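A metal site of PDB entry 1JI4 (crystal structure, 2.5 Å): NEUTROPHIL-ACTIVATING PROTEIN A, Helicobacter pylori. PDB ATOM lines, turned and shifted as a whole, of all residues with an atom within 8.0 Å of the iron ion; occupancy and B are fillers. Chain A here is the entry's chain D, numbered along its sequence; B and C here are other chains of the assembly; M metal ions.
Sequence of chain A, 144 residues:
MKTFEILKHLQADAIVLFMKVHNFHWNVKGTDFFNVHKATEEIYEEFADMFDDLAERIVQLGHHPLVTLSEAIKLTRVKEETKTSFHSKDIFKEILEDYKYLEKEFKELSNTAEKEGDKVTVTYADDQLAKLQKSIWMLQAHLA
The side-chain carboxylate (OE2) of Glu 56 is bound to the iron ion.
The iron ion is bound by NE2 of His 25 of chain B (2.2 Å).
The iron ion is bound by OD2 of Asp 52 (2.2 Å).
The iron ion has three donor atoms within binding distance.
Merely in contact with the iron ion: Tyr 44 of chain B and His 37 of chain B.
The nearest printed residue that does not touch the iron ion is Trp 26 of chain B (4.9 Å).
O of His 25 of chain B lies within hydrogen-bond range of ND1 of His 37 of chain B, 2.8 Å away.
OD1 of Asp 52 is in hydrogen-bond range of NE1 of Trp 26 of chain B, at 2.7 Å.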
ATOM      1  N   ALA A  48      12.316 -12.266  -9.417  1.00  0.00           N
ATOM      2  CA  ALA A  48      12.698 -12.772 -10.725  1.00  0.00           C
ATOM      3  C   ALA A  48      14.196 -13.084 -10.703  1.00  0.00           C
ATOM      4  O   ALA A  48      14.636 -14.085 -11.251  1.00  0.00           O
ATOM      5  CB  ALA A  48      12.384 -11.753 -11.805  1.00  0.00           C
ATOM      6  N   ASP A  49      14.975 -12.215 -10.049  1.00  0.00           N
ATOM      7  CA  ASP A  49      16.420 -12.423  -9.956  1.00  0.00           C
ATOM      8  C   ASP A  49      16.752 -13.599  -9.060  1.00  0.00           C
ATOM      9  O   ASP A  49      17.636 -14.399  -9.372  1.00  0.00           O
ATOM     10  CB  ASP A  49      17.141 -11.191  -9.419  1.00  0.00           C
ATOM     11  CG  ASP A  49      17.249 -10.084 -10.446  1.00  0.00           C
ATOM     12  OD1 ASP A  49      17.363 -10.395 -11.657  1.00  0.00           O
ATOM     13  OD2 ASP A  49      17.221  -8.892 -10.040  1.00  0.00           O
ATOM     14  N   PHE A  51      14.822 -16.116  -8.398  1.00  0.00           N
ATOM     15  CA  PHE A  51      14.357 -17.282  -9.121  1.00  0.00           C
ATOM     16  C   PHE A  51      15.484 -17.791 -10.033  1.00  0.00           C
ATOM     17  O   PHE A  51      15.782 -18.988 -10.078  1.00  0.00           O
ATOM     18  CB  PHE A  51      13.125 -16.879  -9.950  1.00  0.00           C
ATOM     19  CG  PHE A  51      12.593 -17.968 -10.839  1.00  0.00           C
ATOM     20  CD1 PHE A  51      12.090 -19.150 -10.298  1.00  0.00           C
ATOM     21  CD2 PHE A  51      12.563 -17.795 -12.218  1.00  0.00           C
ATOM     22  CE1 PHE A  51      11.556 -20.147 -11.123  1.00  0.00           C
ATOM     23  CE2 PHE A  51      12.020 -18.784 -13.051  1.00  0.00           C
ATOM     24  CZ  PHE A  51      11.517 -19.964 -12.495  1.00  0.00           C
ATOM     25  N   ASP A  52      16.116 -16.868 -10.742  1.00  0.00           N
ATOM     26  CA  ASP A  52      17.190 -17.224 -11.660  1.00  0.00           C
ATOM     27  C   ASP A  52      18.485 -17.662 -10.937  1.00  0.00           C
ATOM     28  O   ASP A  52      19.142 -18.618 -11.358  1.00  0.00           O
ATOM     29  CB  ASP A  52      17.473 -16.054 -12.598  1.00  0.00           C
ATOM     30  CG  ASP A  52      18.339 -16.430 -13.769  1.00  0.00           C
ATOM     31  OD1 ASP A  52      18.023 -17.431 -14.453  1.00  0.00           O
ATOM     32  OD2 ASP A  52      19.340 -15.736 -14.015  1.00  0.00           O
ATOM     33  N   ASP A  53      18.843 -16.984  -9.855  1.00  0.00           N
ATOM     34  CA  ASP A  53      20.040 -17.330  -9.098  1.00  0.00           C
ATOM     35  C   ASP A  53      19.926 -18.697  -8.439  1.00  0.00           C
ATOM     36  O   ASP A  53      20.871 -19.487  -8.469  1.00  0.00           O
ATOM     37  CB  ASP A  53      20.335 -16.294  -8.017  1.00  0.00           C
ATOM     38  CG  ASP A  53      20.747 -14.959  -8.599  1.00  0.00           C
ATOM     39  OD1 ASP A  53      21.426 -14.960  -9.655  1.00  0.00           O
ATOM     40  OD2 ASP A  53      20.405 -13.914  -7.992  1.00  0.00           O
ATOM     41  N   ALA A  55      18.033 -21.229  -9.323  1.00  0.00           N
ATOM     42  CA  ALA A  55      18.066 -22.237 -10.380  1.00  0.00           C
ATOM     43  C   ALA A  55      19.469 -22.501 -10.899  1.00  0.00           C
ATOM     44  O   ALA A  55      19.854 -23.647 -11.120  1.00  0.00           O
ATOM     45  CB  ALA A  55      17.167 -21.816 -11.527  1.00  0.00           C
ATOM     46  N   GLU A  56      20.242 -21.430 -11.106  1.00  0.00           N
ATOM     47  CA  GLU A  56      21.603 -21.596 -11.609  1.00  0.00           C
ATOM     48  C   GLU A  56      22.526 -22.168 -10.547  1.00  0.00           C
ATOM     49  O   GLU A  56      23.492 -22.856 -10.880  1.00  0.00           O
ATOM     50  CB  GLU A  56      22.125 -20.254 -12.133  1.00  0.00           C
ATOM     51  CG  GLU A  56      21.224 -19.701 -13.214  1.00  0.00           C
ATOM     52  CD  GLU A  56      21.759 -18.447 -13.861  1.00  0.00           C
ATOM     53  OE1 GLU A  56      22.469 -17.676 -13.175  1.00  0.00           O
ATOM     54  OE2 GLU A  56      21.447 -18.221 -15.049  1.00  0.00           O
ATOM     55  N   HIS B  22      13.338 -19.818 -19.456  1.00  0.00           N
ATOM     56  CA  HIS B  22      14.291 -19.826 -18.353  1.00  0.00           C
ATOM     57  C   HIS B  22      14.926 -21.214 -18.405  1.00  0.00           C
ATOM     58  O   HIS B  22      16.130 -21.360 -18.245  1.00  0.00           O
ATOM     59  CB  HIS B  22      13.588 -19.634 -17.010  1.00  0.00           C
ATOM     60  CG  HIS B  22      13.566 -18.217 -16.532  1.00  0.00           C
ATOM     61  ND1 HIS B  22      14.582 -17.672 -15.775  1.00  0.00           N
ATOM     62  CD2 HIS B  22      12.643 -17.234 -16.683  1.00  0.00           C
ATOM     63  CE1 HIS B  22      14.279 -16.419 -15.480  1.00  0.00           C
ATOM     64  NE2 HIS B  22      13.113 -16.128 -16.023  1.00  0.00           N
ATOM     65  N   HIS B  25      17.394 -21.221 -20.975  1.00  0.00           N
ATOM     66  CA  HIS B  25      18.427 -20.339 -20.456  1.00  0.00           C
ATOM     67  C   HIS B  25      19.422 -21.064 -19.532  1.00  0.00           C
ATOM     68  O   HIS B  25      20.634 -20.877 -19.631  1.00  0.00           O
ATOM     69  CB  HIS B  25      17.745 -19.203 -19.682  1.00  0.00           C
ATOM     70  CG  HIS B  25      18.679 -18.264 -19.010  1.00  0.00           C
ATOM     71  ND1 HIS B  25      19.434 -17.339 -19.703  1.00  0.00           N
ATOM     72  CD2 HIS B  25      18.946 -18.049 -17.702  1.00  0.00           C
ATOM     73  CE1 HIS B  25      20.116 -16.590 -18.854  1.00  0.00           C
ATOM     74  NE2 HIS B  25      19.837 -17.011 -17.631  1.00  0.00           N
ATOM     75  N   TRP B  26      18.897 -21.888 -18.622  1.00  0.00           N
ATOM     76  CA  TRP B  26      19.743 -22.615 -17.683  1.00  0.00           C
ATOM     77  C   TRP B  26      20.326 -23.902 -18.250  1.00  0.00           C
ATOM     78  O   TRP B  26      21.463 -24.253 -17.948  1.00  0.00           O
ATOM     79  CB  TRP B  26      18.971 -23.041 -16.429  1.00  0.00           C
ATOM     80  CG  TRP B  26      18.190 -21.996 -15.744  1.00  0.00           C
ATOM     81  CD1 TRP B  26      18.599 -20.743 -15.418  1.00  0.00           C
ATOM     82  CD2 TRP B  26      16.857 -22.141 -15.230  1.00  0.00           C
ATOM     83  NE1 TRP B  26      17.598 -20.082 -14.728  1.00  0.00           N
ATOM     84  CE2 TRP B  26      16.517 -20.919 -14.607  1.00  0.00           C
ATOM     85  CE3 TRP B  26      15.913 -23.180 -15.242  1.00  0.00           C
ATOM     86  CZ2 TRP B  26      15.272 -20.707 -13.988  1.00  0.00           C
ATOM     87  CZ3 TRP B  26      14.667 -22.958 -14.624  1.00  0.00           C
ATOM     88  CH2 TRP B  26      14.361 -21.732 -14.010  1.00  0.00           C
ATOM     89  N   HIS B  37      22.345 -18.387 -24.088  1.00  0.00           N
ATOM     90  CA  HIS B  37      22.151 -18.071 -22.681  1.00  0.00           C
ATOM     91  C   HIS B  37      21.812 -16.588 -22.592  1.00  0.00           C
ATOM     92  O   HIS B  37      20.919 -16.187 -21.846  1.00  0.00           O
ATOM     93  CB  HIS B  37      23.441 -18.357 -21.895  1.00  0.00           C
ATOM     94  CG  HIS B  37      23.333 -18.109 -20.424  1.00  0.00           C
ATOM     95  ND1 HIS B  37      22.567 -18.891 -19.581  1.00  0.00           N
ATOM     96  CD2 HIS B  37      23.910 -17.170 -19.628  1.00  0.00           C
ATOM     97  CE1 HIS B  37      22.678 -18.447 -18.344  1.00  0.00           C
ATOM     98  NE2 HIS B  37      23.484 -17.402 -18.348  1.00  0.00           N
ATOM     99  N   LYS B  38      22.513 -15.779 -23.386  1.00  0.00           N
ATOM    100  CA  LYS B  38      22.313 -14.335 -23.441  1.00  0.00           C
ATOM    101  C   LYS B  38      20.981 -13.956 -24.104  1.00  0.00           C
ATOM    102  O   LYS B  38      20.268 -13.072 -23.626  1.00  0.00           O
ATOM    103  CB  LYS B  38      23.480 -13.700 -24.208  1.00  0.00           C
ATOM    104  CG  LYS B  38      23.440 -12.184 -24.296  1.00  0.00           C
ATOM    105  CD  LYS B  38      23.576 -11.561 -22.916  1.00  0.00           C
ATOM    106  CE  LYS B  38      23.500 -10.034 -22.967  1.00  0.00           C
ATOM    107  NZ  LYS B  38      23.705  -9.444 -21.607  1.00  0.00           N
ATOM    108  N   THR B  40      18.193 -15.888 -24.566  1.00  0.00           N
ATOM    109  CA  THR B  40      17.040 -16.336 -23.799  1.00  0.00           C
ATOM    110  C   THR B  40      16.728 -15.379 -22.643  1.00  0.00           C
ATOM    111  O   THR B  40      15.581 -15.206 -22.258  1.00  0.00           O
ATOM    112  CB  THR B  40      17.222 -17.772 -23.251  1.00  0.00           C
ATOM    113  OG1 THR B  40      18.482 -17.863 -22.572  1.00  0.00           O
ATOM    114  CG2 THR B  40      17.178 -18.785 -24.390  1.00  0.00           C
ATOM    115  N   GLU B  41      17.768 -14.758 -22.092  1.00  0.00           N
ATOM    116  CA  GLU B  41      17.532 -13.808 -21.002  1.00  0.00           C
ATOM    117  C   GLU B  41      16.748 -12.601 -21.523  1.00  0.00           C
ATOM    118  O   GLU B  41      15.818 -12.139 -20.878  1.00  0.00           O
ATOM    119  CB  GLU B  41      18.843 -13.339 -20.397  1.00  0.00           C
ATOM    120  CG  GLU B  41      18.628 -12.209 -19.422  1.00  0.00           C
ATOM    121  CD  GLU B  41      19.921 -11.648 -18.873  1.00  0.00           C
ATOM    122  OE1 GLU B  41      20.866 -11.443 -19.664  1.00  0.00           O
ATOM    123  OE2 GLU B  41      19.982 -11.399 -17.654  1.00  0.00           O
ATOM    124  N   TYR B  44      13.027 -13.761 -22.025  1.00  0.00           N
ATOM    125  CA  TYR B  44      12.142 -13.861 -20.859  1.00  0.00           C
ATOM    126  C   TYR B  44      11.930 -12.516 -20.175  1.00  0.00           C
ATOM    127  O   TYR B  44      10.940 -12.330 -19.463  1.00  0.00           O
ATOM    128  CB  TYR B  44      12.596 -14.952 -19.867  1.00  0.00           C
ATOM    129  CG  TYR B  44      13.902 -14.760 -19.119  1.00  0.00           C
ATOM    130  CD1 TYR B  44      14.092 -13.663 -18.280  1.00  0.00           C
ATOM    131  CD2 TYR B  44      14.914 -15.720 -19.198  1.00  0.00           C
ATOM    132  CE1 TYR B  44      15.259 -13.534 -17.523  1.00  0.00           C
ATOM    133  CE2 TYR B  44      16.082 -15.600 -18.440  1.00  0.00           C
ATOM    134  CZ  TYR B  44      16.242 -14.499 -17.599  1.00  0.00           C
ATOM    135  OH  TYR B  44      17.383 -14.381 -16.825  1.00  0.00           O
ATOM    136  N   LYS C 134      30.734 -20.607 -11.059  1.00  0.00           N
ATOM    137  CA  LYS C 134      29.758 -20.231 -12.074  1.00  0.00           C
ATOM    138  C   LYS C 134      30.384 -20.411 -13.458  1.00  0.00           C
ATOM    139  O   LYS C 134      29.746 -20.917 -14.375  1.00  0.00           O
ATOM    140  CB  LYS C 134      29.316 -18.782 -11.890  1.00  0.00           C
ATOM    141  CG  LYS C 134      28.285 -18.334 -12.913  1.00  0.00           C
ATOM    142  CD  LYS C 134      27.687 -16.997 -12.546  1.00  0.00           C
ATOM    143  CE  LYS C 134      26.530 -16.658 -13.469  1.00  0.00           C
ATOM    144  NZ  LYS C 134      25.790 -15.436 -13.028  1.00  0.00           N
ATOM    145  N   TRP C 137      30.776 -24.092 -14.494  1.00  0.00           N
ATOM    146  CA  TRP C 137      29.508 -24.612 -15.007  1.00  0.00           C
ATOM    147  C   TRP C 137      29.380 -24.224 -16.486  1.00  0.00           C
ATOM    148  O   TRP C 137      29.159 -25.081 -17.339  1.00  0.00           O
ATOM    149  CB  TRP C 137      28.328 -24.046 -14.208  1.00  0.00           C
ATOM    150  CG  TRP C 137      27.040 -23.915 -15.007  1.00  0.00           C
ATOM    151  CD1 TRP C 137      26.470 -24.865 -15.823  1.00  0.00           C
ATOM    152  CD2 TRP C 137      26.199 -22.748 -15.111  1.00  0.00           C
ATOM    153  NE1 TRP C 137      25.346 -24.360 -16.421  1.00  0.00           N
ATOM    154  CE2 TRP C 137      25.151 -23.064 -16.017  1.00  0.00           C
ATOM    155  CE3 TRP C 137      26.234 -21.471 -14.542  1.00  0.00           C
ATOM    156  CZ2 TRP C 137      24.147 -22.152 -16.347  1.00  0.00           C
ATOM    157  CZ3 TRP C 137      25.236 -20.559 -14.880  1.00  0.00           C
ATOM    158  CH2 TRP C 137      24.208 -20.902 -15.782  1.00  0.00           C
HETATM  159 FE    FE M   1      20.637 -16.312 -15.713  1.00  0.00          FE
